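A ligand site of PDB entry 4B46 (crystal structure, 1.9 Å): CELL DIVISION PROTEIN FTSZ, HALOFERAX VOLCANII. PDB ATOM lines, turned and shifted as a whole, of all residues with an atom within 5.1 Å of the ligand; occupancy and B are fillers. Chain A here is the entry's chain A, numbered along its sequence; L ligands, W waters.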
ATOM      1  N   PHE A   8      34.513   2.216 -18.673  1.00  0.00           N
ATOM      2  CA  PHE A   8      33.847   0.915 -18.814  1.00  0.00           C
ATOM      3  C   PHE A   8      33.198   0.832 -20.189  1.00  0.00           C
ATOM      4  O   PHE A   8      32.393   1.692 -20.553  1.00  0.00           O
ATOM      5  CB  PHE A   8      32.780   0.732 -17.719  1.00  0.00           C
ATOM      6  CG  PHE A   8      32.791  -0.634 -17.072  1.00  0.00           C
ATOM      7  CD1 PHE A   8      32.441  -1.757 -17.808  1.00  0.00           C
ATOM      8  CD2 PHE A   8      33.143  -0.797 -15.752  1.00  0.00           C
ATOM      9  CE1 PHE A   8      32.448  -3.020 -17.228  1.00  0.00           C
ATOM     10  CE2 PHE A   8      33.159  -2.058 -15.154  1.00  0.00           C
ATOM     11  CZ  PHE A   8      32.803  -3.171 -15.899  1.00  0.00           C
ATOM     12  N   GLY A   9      33.558  -0.201 -20.956  1.00  0.00           N
ATOM     13  CA  GLY A   9      33.068  -0.297 -22.323  1.00  0.00           C
ATOM     14  C   GLY A   9      33.915   0.551 -23.262  1.00  0.00           C
ATOM     15  O   GLY A   9      34.839   1.240 -22.827  1.00  0.00           O
ATOM     16  N   GLN A  10      33.595   0.525 -24.545  1.00  0.00           N
ATOM     17  CA  GLN A  10      34.433   1.196 -25.539  1.00  0.00           C
ATOM     18  C   GLN A  10      34.434   2.728 -25.414  1.00  0.00           C
ATOM     19  O   GLN A  10      35.495   3.356 -25.476  1.00  0.00           O
ATOM     20  CB  GLN A  10      34.046   0.765 -26.957  1.00  0.00           C
ATOM     21  CG  GLN A  10      34.937   1.379 -28.006  1.00  0.00           C
ATOM     22  CD  GLN A  10      34.487   1.077 -29.417  1.00  0.00           C
ATOM     23  OE1 GLN A  10      33.373   0.626 -29.643  1.00  0.00           O
ATOM     24  NE2 GLN A  10      35.360   1.334 -30.384  1.00  0.00           N
ATOM     25  N   ALA A  11      33.265   3.317 -25.250  1.00  0.00           N
ATOM     26  CA  ALA A  11      33.129   4.773 -25.090  1.00  0.00           C
ATOM     27  C   ALA A  11      33.832   5.283 -23.825  1.00  0.00           C
ATOM     28  O   ALA A  11      34.616   6.224 -23.866  1.00  0.00           O
ATOM     29  CB  ALA A  11      31.659   5.179 -25.065  1.00  0.00           C
ATOM     30  N   GLY A  12      33.519   4.654 -22.692  1.00  0.00           N
ATOM     31  CA  GLY A  12      34.147   5.001 -21.426  1.00  0.00           C
ATOM     32  C   GLY A  12      35.656   4.936 -21.522  1.00  0.00           C
ATOM     33  O   GLY A  12      36.354   5.806 -21.010  1.00  0.00           O
ATOM     34  N   LYS A  14      37.569   5.248 -24.282  1.00  0.00           N
ATOM     35  CA  LYS A  14      38.092   6.304 -25.141  1.00  0.00           C
ATOM     36  C   LYS A  14      38.076   7.657 -24.432  1.00  0.00           C
ATOM     37  O   LYS A  14      38.971   8.483 -24.598  1.00  0.00           O
ATOM     38  CB  LYS A  14      37.317   6.364 -26.466  1.00  0.00           C
ATOM     39  CG  LYS A  14      37.562   5.162 -27.370  1.00  0.00           C
ATOM     40  CD  LYS A  14      36.547   5.079 -28.496  1.00  0.00           C
ATOM     41  CE  LYS A  14      36.613   6.283 -29.414  1.00  0.00           C
ATOM     42  NZ  LYS A  14      35.574   6.234 -30.485  1.00  0.00           N
ATOM     43  N   VAL A  15      37.042   7.888 -23.639  1.00  0.00           N
ATOM     44  CA  VAL A  15      36.923   9.154 -22.922  1.00  0.00           C
ATOM     45  C   VAL A  15      37.995   9.262 -21.829  1.00  0.00           C
ATOM     46  O   VAL A  15      38.655  10.295 -21.713  1.00  0.00           O
ATOM     47  CB  VAL A  15      35.499   9.346 -22.363  1.00  0.00           C
ATOM     48  CG1 VAL A  15      35.437  10.550 -21.384  1.00  0.00           C
ATOM     49  CG2 VAL A  15      34.520   9.530 -23.537  1.00  0.00           C
ATOM     50  N   ASN A  38      36.830  -3.712 -20.235  1.00  0.00           N
ATOM     51  CA  ASN A  38      36.053  -4.045 -21.425  1.00  0.00           C
ATOM     52  C   ASN A  38      35.976  -5.553 -21.613  1.00  0.00           C
ATOM     53  O   ASN A  38      36.743  -6.303 -20.992  1.00  0.00           O
ATOM     54  CB  ASN A  38      36.629  -3.351 -22.669  1.00  0.00           C
ATOM     55  CG  ASN A  38      35.570  -3.075 -23.754  1.00  0.00           C
ATOM     56  OD1 ASN A  38      34.605  -3.830 -23.934  1.00  0.00           O
ATOM     57  ND2 ASN A  38      35.759  -1.978 -24.499  1.00  0.00           N
ATOM     58  N   ASP A  43      39.168  -3.374 -28.459  1.00  0.00           N
ATOM     59  CA  ASP A  43      38.971  -2.031 -27.892  1.00  0.00           C
ATOM     60  C   ASP A  43      40.102  -1.639 -26.964  1.00  0.00           C
ATOM     61  O   ASP A  43      40.604  -0.508 -27.026  1.00  0.00           O
ATOM     62  CB  ASP A  43      37.645  -1.932 -27.135  1.00  0.00           C
ATOM     63  CG  ASP A  43      36.435  -2.128 -28.031  1.00  0.00           C
ATOM     64  OD1 ASP A  43      36.621  -2.279 -29.260  1.00  0.00           O
ATOM     65  OD2 ASP A  43      35.288  -2.135 -27.527  1.00  0.00           O
ATOM     66  N   VAL A  68      30.004  -8.033 -25.639  1.00  0.00           N
ATOM     67  CA  VAL A  68      28.648  -8.508 -25.428  1.00  0.00           C
ATOM     68  C   VAL A  68      27.678  -7.801 -26.370  1.00  0.00           C
ATOM     69  O   VAL A  68      26.465  -7.943 -26.236  1.00  0.00           O
ATOM     70  CB  VAL A  68      28.176  -8.306 -23.974  1.00  0.00           C
ATOM     71  CG1 VAL A  68      29.155  -8.950 -22.987  1.00  0.00           C
ATOM     72  CG2 VAL A  68      27.968  -6.839 -23.664  1.00  0.00           C
ATOM     73  N   GLY A  69      28.223  -7.057 -27.330  1.00  0.00           N
ATOM     74  CA  GLY A  69      27.386  -6.288 -28.236  1.00  0.00           C
ATOM     75  C   GLY A  69      26.610  -5.275 -27.405  1.00  0.00           C
ATOM     76  O   GLY A  69      27.200  -4.548 -26.605  1.00  0.00           O
ATOM     77  N   GLY A 106      29.375   4.829 -21.639  1.00  0.00           N
ATOM     78  CA  GLY A 106      28.216   5.056 -22.485  1.00  0.00           C
ATOM     79  C   GLY A 106      27.099   4.190 -21.935  1.00  0.00           C
ATOM     80  O   GLY A 106      27.346   3.080 -21.465  1.00  0.00           O
ATOM     81  N   LEU A 107      25.873   4.686 -21.957  1.00  0.00           N
ATOM     82  CA  LEU A 107      24.785   3.920 -21.354  1.00  0.00           C
ATOM     83  C   LEU A 107      23.989   3.116 -22.390  1.00  0.00           C
ATOM     84  O   LEU A 107      23.179   2.267 -22.039  1.00  0.00           O
ATOM     85  CB  LEU A 107      23.850   4.823 -20.541  1.00  0.00           C
ATOM     86  CG  LEU A 107      24.556   5.592 -19.409  1.00  0.00           C
ATOM     87  CD1 LEU A 107      23.514   6.190 -18.505  1.00  0.00           C
ATOM     88  CD2 LEU A 107      25.483   4.682 -18.615  1.00  0.00           C
ATOM     89  N   GLY A 108      24.256   3.366 -23.672  1.00  0.00           N
ATOM     90  CA  GLY A 108      23.447   2.787 -24.737  1.00  0.00           C
ATOM     91  C   GLY A 108      23.846   1.388 -25.178  1.00  0.00           C
ATOM     92  O   GLY A 108      23.086   0.743 -25.909  1.00  0.00           O
ATOM     93  N   GLY A 109      25.024   0.915 -24.747  1.00  0.00           N
ATOM     94  CA  GLY A 109      25.566  -0.357 -25.209  1.00  0.00           C
ATOM     95  C   GLY A 109      25.365  -1.532 -24.268  1.00  0.00           C
ATOM     96  O   GLY A 109      24.322  -1.650 -23.625  1.00  0.00           O
ATOM     97  N   GLY A 110      26.355  -2.415 -24.170  1.00  0.00           N
ATOM     98  CA  GLY A 110      26.220  -3.593 -23.342  1.00  0.00           C
ATOM     99  C   GLY A 110      27.204  -3.703 -22.190  1.00  0.00           C
ATOM    100  O   GLY A 110      26.814  -3.960 -21.047  1.00  0.00           O
ATOM    101  N   THR A 111      28.486  -3.522 -22.478  1.00  0.00           N
ATOM    102  CA  THR A 111      29.534  -3.727 -21.486  1.00  0.00           C
ATOM    103  C   THR A 111      29.495  -2.632 -20.428  1.00  0.00           C
ATOM    104  O   THR A 111      29.368  -2.919 -19.227  1.00  0.00           O
ATOM    105  CB  THR A 111      30.908  -3.806 -22.168  1.00  0.00           C
ATOM    106  OG1 THR A 111      30.963  -4.973 -22.975  1.00  0.00           O
ATOM    107  CG2 THR A 111      32.029  -3.891 -21.136  1.00  0.00           C
ATOM    108  N   GLY A 112      29.594  -1.387 -20.869  1.00  0.00           N
ATOM    109  CA  GLY A 112      29.562  -0.247 -19.968  1.00  0.00           C
ATOM    110  C   GLY A 112      28.191  -0.074 -19.344  1.00  0.00           C
ATOM    111  O   GLY A 112      28.068   0.134 -18.143  1.00  0.00           O
ATOM    112  N   SER A 113      27.167  -0.174 -20.178  1.00  0.00           N
ATOM    113  CA  SER A 113      25.779  -0.013 -19.737  1.00  0.00           C
ATOM    114  C   SER A 113      25.446  -0.936 -18.561  1.00  0.00           C
ATOM    115  O   SER A 113      24.867  -0.505 -17.553  1.00  0.00           O
ATOM    116  CB  SER A 113      24.862  -0.298 -20.925  1.00  0.00           C
ATOM    117  OG  SER A 113      23.490  -0.265 -20.557  1.00  0.00           O
ATOM    118  N   ILE A 136      27.089   8.638 -20.346  1.00  0.00           N
ATOM    119  CA  ILE A 136      26.952   9.264 -21.638  1.00  0.00           C
ATOM    120  C   ILE A 136      25.738   8.684 -22.377  1.00  0.00           C
ATOM    121  O   ILE A 136      25.706   7.487 -22.681  1.00  0.00           O
ATOM    122  CB  ILE A 136      28.214   9.058 -22.474  1.00  0.00           C
ATOM    123  CG1 ILE A 136      29.412   9.748 -21.798  1.00  0.00           C
ATOM    124  CG2 ILE A 136      27.994   9.532 -23.900  1.00  0.00           C
ATOM    125  CD1 ILE A 136      30.765   9.302 -22.325  1.00  0.00           C
ATOM    126  N   LEU A 137      24.733   9.535 -22.622  1.00  0.00           N
ATOM    127  CA  LEU A 137      23.486   9.089 -23.233  1.00  0.00           C
ATOM    128  C   LEU A 137      23.632   8.995 -24.742  1.00  0.00           C
ATOM    129  O   LEU A 137      24.431   9.722 -25.336  1.00  0.00           O
ATOM    130  CB  LEU A 137      22.334  10.050 -22.891  1.00  0.00           C
ATOM    131  CG  LEU A 137      22.088  10.234 -21.396  1.00  0.00           C
ATOM    132  CD1 LEU A 137      20.871  11.129 -21.138  1.00  0.00           C
ATOM    133  CD2 LEU A 137      21.934   8.889 -20.722  1.00  0.00           C
ATOM    134  N   PRO A 138      22.865   8.089 -25.373  1.00  0.00           N
ATOM    135  CA  PRO A 138      23.044   7.847 -26.804  1.00  0.00           C
ATOM    136  C   PRO A 138      22.378   8.904 -27.672  1.00  0.00           C
ATOM    137  O   PRO A 138      21.532   9.669 -27.186  1.00  0.00           O
ATOM    138  CB  PRO A 138      22.349   6.489 -27.024  1.00  0.00           C
ATOM    139  CG  PRO A 138      21.274   6.459 -25.999  1.00  0.00           C
ATOM    140  CD  PRO A 138      21.876   7.172 -24.783  1.00  0.00           C
ATOM    141  N   GLY A 139      22.768   8.936 -28.938  1.00  0.00           N
ATOM    142  CA  GLY A 139      22.087   9.755 -29.920  1.00  0.00           C
ATOM    143  C   GLY A 139      20.777   9.094 -30.280  1.00  0.00           C
ATOM    144  O   GLY A 139      20.685   7.869 -30.345  1.00  0.00           O
ATOM    145  N   GLU A 142      20.663   6.426 -33.081  1.00  0.00           N
ATOM    146  CA  GLU A 142      21.312   5.110 -32.970  1.00  0.00           C
ATOM    147  C   GLU A 142      20.351   3.944 -33.140  1.00  0.00           C
ATOM    148  O   GLU A 142      20.687   2.965 -33.799  1.00  0.00           O
ATOM    149  CB  GLU A 142      22.071   4.984 -31.640  1.00  0.00           C
ATOM    150  CG  GLU A 142      23.154   6.025 -31.476  1.00  0.00           C
ATOM    151  CD  GLU A 142      24.042   5.747 -30.277  1.00  0.00           C
ATOM    152  OE1 GLU A 142      24.365   4.576 -30.034  1.00  0.00           O
ATOM    153  OE2 GLU A 142      24.391   6.715 -29.570  1.00  0.00           O
ATOM    154  N   TYR A 146      19.306   1.009 -28.251  1.00  0.00           N
ATOM    155  CA  TYR A 146      20.284   1.799 -27.525  1.00  0.00           C
ATOM    156  C   TYR A 146      19.614   2.753 -26.551  1.00  0.00           C
ATOM    157  O   TYR A 146      20.099   2.945 -25.443  1.00  0.00           O
ATOM    158  CB  TYR A 146      21.243   2.500 -28.496  1.00  0.00           C
ATOM    159  CG  TYR A 146      21.732   1.492 -29.505  1.00  0.00           C
ATOM    160  CD1 TYR A 146      22.716   0.552 -29.170  1.00  0.00           C
ATOM    161  CD2 TYR A 146      21.165   1.427 -30.766  1.00  0.00           C
ATOM    162  CE1 TYR A 146      23.135  -0.423 -30.100  1.00  0.00           C
ATOM    163  CE2 TYR A 146      21.570   0.470 -31.692  1.00  0.00           C
ATOM    164  CZ  TYR A 146      22.556  -0.439 -31.361  1.00  0.00           C
ATOM    165  OH  TYR A 146      22.945  -1.369 -32.303  1.00  0.00           O
ATOM    166  N   ASN A 169      24.907  12.571 -25.723  1.00  0.00           N
ATOM    167  CA  ASN A 169      25.318  12.610 -27.137  1.00  0.00           C
ATOM    168  C   ASN A 169      24.247  13.189 -28.045  1.00  0.00           C
ATOM    169  O   ASN A 169      24.560  13.796 -29.062  1.00  0.00           O
ATOM    170  CB  ASN A 169      25.687  11.227 -27.666  1.00  0.00           C
ATOM    171  CG  ASN A 169      27.052  10.747 -27.196  1.00  0.00           C
ATOM    172  OD1 ASN A 169      27.839  11.524 -26.630  1.00  0.00           O
ATOM    173  ND2 ASN A 169      27.342   9.483 -27.436  1.00  0.00           N
ATOM    174  N   GLN A 180      32.564   7.955 -36.201  1.00  0.00           N
ATOM    175  CA  GLN A 180      33.776   7.978 -35.400  1.00  0.00           C
ATOM    176  C   GLN A 180      34.371   9.387 -35.337  1.00  0.00           C
ATOM    177  O   GLN A 180      34.886   9.792 -34.291  1.00  0.00           O
ATOM    178  CB  GLN A 180      34.799   6.989 -35.966  1.00  0.00           C
ATOM    179  CG  GLN A 180      35.969   6.732 -35.010  1.00  0.00           C
ATOM    180  CD  GLN A 180      35.494   6.348 -33.614  1.00  0.00           C
ATOM    181  OE1 GLN A 180      35.889   6.973 -32.620  1.00  0.00           O
ATOM    182  NE2 GLN A 180      34.641   5.317 -33.527  1.00  0.00           N
ATOM    183  N   TYR A 183      32.474  11.242 -32.771  1.00  0.00           N
ATOM    184  CA  TYR A 183      32.878  10.876 -31.409  1.00  0.00           C
ATOM    185  C   TYR A 183      34.186  11.535 -30.991  1.00  0.00           C
ATOM    186  O   TYR A 183      34.333  11.933 -29.829  1.00  0.00           O
ATOM    187  CB  TYR A 183      32.967   9.351 -31.241  1.00  0.00           C
ATOM    188  CG  TYR A 183      31.623   8.655 -31.192  1.00  0.00           C
ATOM    189  CD1 TYR A 183      30.537   9.246 -30.561  1.00  0.00           C
ATOM    190  CD2 TYR A 183      31.438   7.405 -31.774  1.00  0.00           C
ATOM    191  CE1 TYR A 183      29.297   8.616 -30.506  1.00  0.00           C
ATOM    192  CE2 TYR A 183      30.208   6.767 -31.724  1.00  0.00           C
ATOM    193  CZ  TYR A 183      29.139   7.384 -31.093  1.00  0.00           C
ATOM    194  OH  TYR A 183      27.921   6.759 -31.039  1.00  0.00           O
ATOM    195  N   ILE A 186      33.200  15.017 -30.098  1.00  0.00           N
ATOM    196  CA  ILE A 186      32.410  14.961 -28.868  1.00  0.00           C
ATOM    197  C   ILE A 186      33.275  14.666 -27.633  1.00  0.00           C
ATOM    198  O   ILE A 186      33.127  15.303 -26.580  1.00  0.00           O
ATOM    199  CB  ILE A 186      31.270  13.935 -28.959  1.00  0.00           C
ATOM    200  CG1 ILE A 186      30.197  14.433 -29.948  1.00  0.00           C
ATOM    201  CG2 ILE A 186      30.656  13.682 -27.584  1.00  0.00           C
ATOM    202  CD1 ILE A 186      29.187  13.362 -30.375  1.00  0.00           C
ATOM    203  N   ASN A 187      34.204  13.720 -27.779  1.00  0.00           N
ATOM    204  CA  ASN A 187      35.084  13.390 -26.661  1.00  0.00           C
ATOM    205  C   ASN A 187      35.977  14.566 -26.230  1.00  0.00           C
ATOM    206  O   ASN A 187      36.291  14.695 -25.058  1.00  0.00           O
ATOM    207  CB  ASN A 187      35.949  12.153 -26.969  1.00  0.00           C
ATOM    208  CG  ASN A 187      35.112  10.894 -27.125  1.00  0.00           C
ATOM    209  OD1 ASN A 187      33.941  10.872 -26.777  1.00  0.00           O
ATOM    210  ND2 ASN A 187      35.728   9.826 -27.638  1.00  0.00           N
ATOM    211  N   ILE A 190      33.687  16.758 -24.198  1.00  0.00           N
ATOM    212  CA  ILE A 190      33.486  16.163 -22.889  1.00  0.00           C
ATOM    213  C   ILE A 190      34.674  16.487 -21.973  1.00  0.00           C
ATOM    214  O   ILE A 190      34.500  16.993 -20.858  1.00  0.00           O
ATOM    215  CB  ILE A 190      33.311  14.630 -22.989  1.00  0.00           C
ATOM    216  CG1 ILE A 190      31.952  14.302 -23.645  1.00  0.00           C
ATOM    217  CG2 ILE A 190      33.474  13.979 -21.640  1.00  0.00           C
ATOM    218  CD1 ILE A 190      31.743  12.806 -23.959  1.00  0.00           C
HETATM  219  P1  LIG L   1      29.963  -1.038 -24.874  1.00  0.00           P
HETATM  220  O1  LIG L   1      29.208  -2.318 -25.083  1.00  0.00           O
HETATM  221  O2  LIG L   1      31.448  -1.210 -25.105  1.00  0.00           O
HETATM  222  O3  LIG L   1      29.671  -0.544 -23.491  1.00  0.00           O
HETATM  223  O4  LIG L   1      29.352  -0.046 -25.969  1.00  0.00           O
HETATM  224  P2  LIG L   1      30.078   1.280 -26.488  1.00  0.00           P
HETATM  225  O5  LIG L   1      30.836   1.960 -25.408  1.00  0.00           O
HETATM  226  O6  LIG L   1      30.932   0.961 -27.688  1.00  0.00           O
HETATM  227  O7  LIG L   1      28.800   2.141 -26.967  1.00  0.00           O
HETATM  228  C1  LIG L   1      27.838   2.500 -25.965  1.00  0.00           C
HETATM  229  C2  LIG L   1      27.252   3.866 -26.297  1.00  0.00           C
HETATM  230  O8  LIG L   1      28.249   4.866 -26.139  1.00  0.00           O
HETATM  231  C3  LIG L   1      26.878   3.984 -27.760  1.00  0.00           C
HETATM  232  O9  LIG L   1      25.529   3.547 -27.897  1.00  0.00           O
HETATM  233  C4  LIG L   1      27.044   5.460 -28.080  1.00  0.00           C
HETATM  234  O10 LIG L   1      25.904   6.195 -27.629  1.00  0.00           O
HETATM  235  C5  LIG L   1      28.123   5.901 -27.142  1.00  0.00           C
HETATM  236  N1  LIG L   1      29.492   5.973 -27.679  1.00  0.00           N
HETATM  237  C6  LIG L   1      30.191   4.989 -28.279  1.00  0.00           C
HETATM  238  N2  LIG L   1      31.456   5.413 -28.551  1.00  0.00           N
HETATM  239  C7  LIG L   1      31.571   6.688 -28.083  1.00  0.00           C
HETATM  240  C8  LIG L   1      32.624   7.713 -28.003  1.00  0.00           C
HETATM  241  O11 LIG L   1      33.771   7.515 -28.472  1.00  0.00           O
HETATM  242  N3  LIG L   1      32.299   8.881 -27.428  1.00  0.00           N
HETATM  243  C9  LIG L   1      31.086   9.145 -26.919  1.00  0.00           C
HETATM  244  N4  LIG L   1      30.856  10.356 -26.365  1.00  0.00           N
HETATM  245  N5  LIG L   1      30.075   8.242 -26.933  1.00  0.00           N
HETATM  246  C10 LIG L   1      30.268   7.032 -27.491  1.00  0.00           C
HETATM  247  O   HOH W   1      26.853   1.129 -29.769  1.00  0.00           O
HETATM  248  O   HOH W   2      30.539  -5.146 -25.630  1.00  0.00           O
HETATM  249  O   HOH W   3      31.163  -1.611 -28.750  1.00  0.00           O
HETATM  250  O   HOH W   4      31.075   2.713 -22.550  1.00  0.00           O
HETATM  251  O   HOH W   5      27.492   0.690 -22.956  1.00  0.00           O
HETATM  252  O   HOH W   6      29.910   1.895 -30.138  1.00  0.00           O
HETATM  253  O   HOH W   7      33.379   4.644 -30.536  1.00  0.00           O
HETATM  254  O   HOH W   8      32.545  -3.517 -25.710  1.00  0.00           O
HETATM  255  O   HOH W   9      25.249   5.929 -24.777  1.00  0.00           O
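The side-chain carboxylate (OE2) of Glu 142 sits at hydrogen-bond distance from an oxygen (O10) of the ligand (2.5 Å).
OD1 of Asn 187 lies within hydrogen-bond range of N3 of the ligand (2.7 Å).
An oxygen (O3) of the ligand lies within hydrogen-bond range of the backbone NH of Gly 112 (2.8 Å).
The backbone NH (N) of Ala 11 is in hydrogen-bond range of an oxygen (O5) of the ligand (2.8 Å).
An oxygen (O2) of the ligand is in hydrogen-bond range of the backbone NH (N) of Gln 10 (2.8 Å).
The side-chain amide oxygen of Gln 10 sits close to an oxygen (O6) of the ligand, 3.1 Å away.
The backbone NH of Thr 111 sits at hydrogen-bond distance from an oxygen (O1) of the ligand.
An oxygen (O11) of the ligand sits at hydrogen-bond distance from the side-chain amino group (NZ) of Lys 14, at 3.0 Å.
O1 of the ligand is in hydrogen-bond range of N of Gly 110 (3.0 Å).
The side-chain amide nitrogen (ND2) of Asn 169 is in hydrogen-bond range of a nitrogen (N5) of the ligand (3.0 Å).
The backbone NH of Gly 139 lies within hydrogen-bond range of the side-chain carboxylate of Glu 142.
O of Tyr 183 sits close to OD1 of Asn 187.
The backbone NH of Gln 10 lies close to the side-chain amide nitrogen of Asn 38, 3.3 Å away.
NE2 of Gln 180 sits close to NZ of Lys 14, at 3.3 Å.
The backbone carbonyl oxygen (O) of Gly 69 sits at hydrogen-bond distance from the backbone NH (N) of Gly 110 (3.3 Å).
The backbone carbonyl oxygen of Leu 137 lies within hydrogen-bond range of the backbone NH of Asn 169.
The backbone carbonyl oxygen of Gly 109 lies close to the side-chain hydroxyl of Ser 113, 3.5 Å away.
The backbone carbonyl oxygen (O) of Ile 136 sits at hydrogen-bond distance from the backbone NH (N) of Leu 107, 2.9 Å away.
O1 of the ligand lies close to O of Gly 69 (3.4 Å).
Residues that only touch the ligand: Gly 9 (3.3 Å), Gly 106 (3.7 Å), Gly 108 (3.9 Å), Gly 109 (3.5 Å), Ile 136 (3.9 Å), Pro 138 (3.4 Å), Tyr 183 (3.3 Å), Ile 186 (3.5 Å) and Ile 190 (3.5 Å).
Hydrophobic or aromatic side chains that line the ligand: Ala 11, Ile 136, Pro 138, Tyr 183, Ile 186 and Ile 190.
Within 4 Å of the ligand: Gly 9, Gln 10, Ala 11, Lys 14, Gly 69, Gly 106, Gly 108, Gly 109, Gly 110, Thr 111, Gly 112, Ile 136, Pro 138, Glu 142, Asn 169, Tyr 183, Ile 186, Asn 187 and Ile 190.
The nearest printed residue that does not touch the ligand is Ser 113 (4.2 Å).
Water W5 lies within hydrogen-bond range of O3 of the ligand (2.6 Å), O of Gly 106 (2.8 Å), N of Ser 113 (2.9 Å) and N of Gly 109 (3.1 Å).
Water W3 lies within hydrogen-bond range of an oxygen (O6) of the ligand and the side-chain amide oxygen of Gln 10.
Water W7 lies within hydrogen-bond range of the side-chain amino group (NZ) of Lys 14, a nitrogen (N2) of the ligand and the side-chain amide nitrogen (NE2) of Gln 180.
Water W9 lies within hydrogen-bond range of O of Ile 136 (2.7 Å), O10 of the ligand (2.9 Å), N of Gly 108 (3.0 Å) and N of Leu 107 (3.1 Å).
Water W4 lies within hydrogen-bond range of O of Phe 8 (2.6 Å), N of Gly 106 (2.9 Å), O5 of the ligand (3.0 Å) and N of Gly 12 (3.1 Å).
Water W2 lies within hydrogen-bond range of OG1 of Thr 111, N of Val 68, O1 of the ligand and N of Gly 69.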
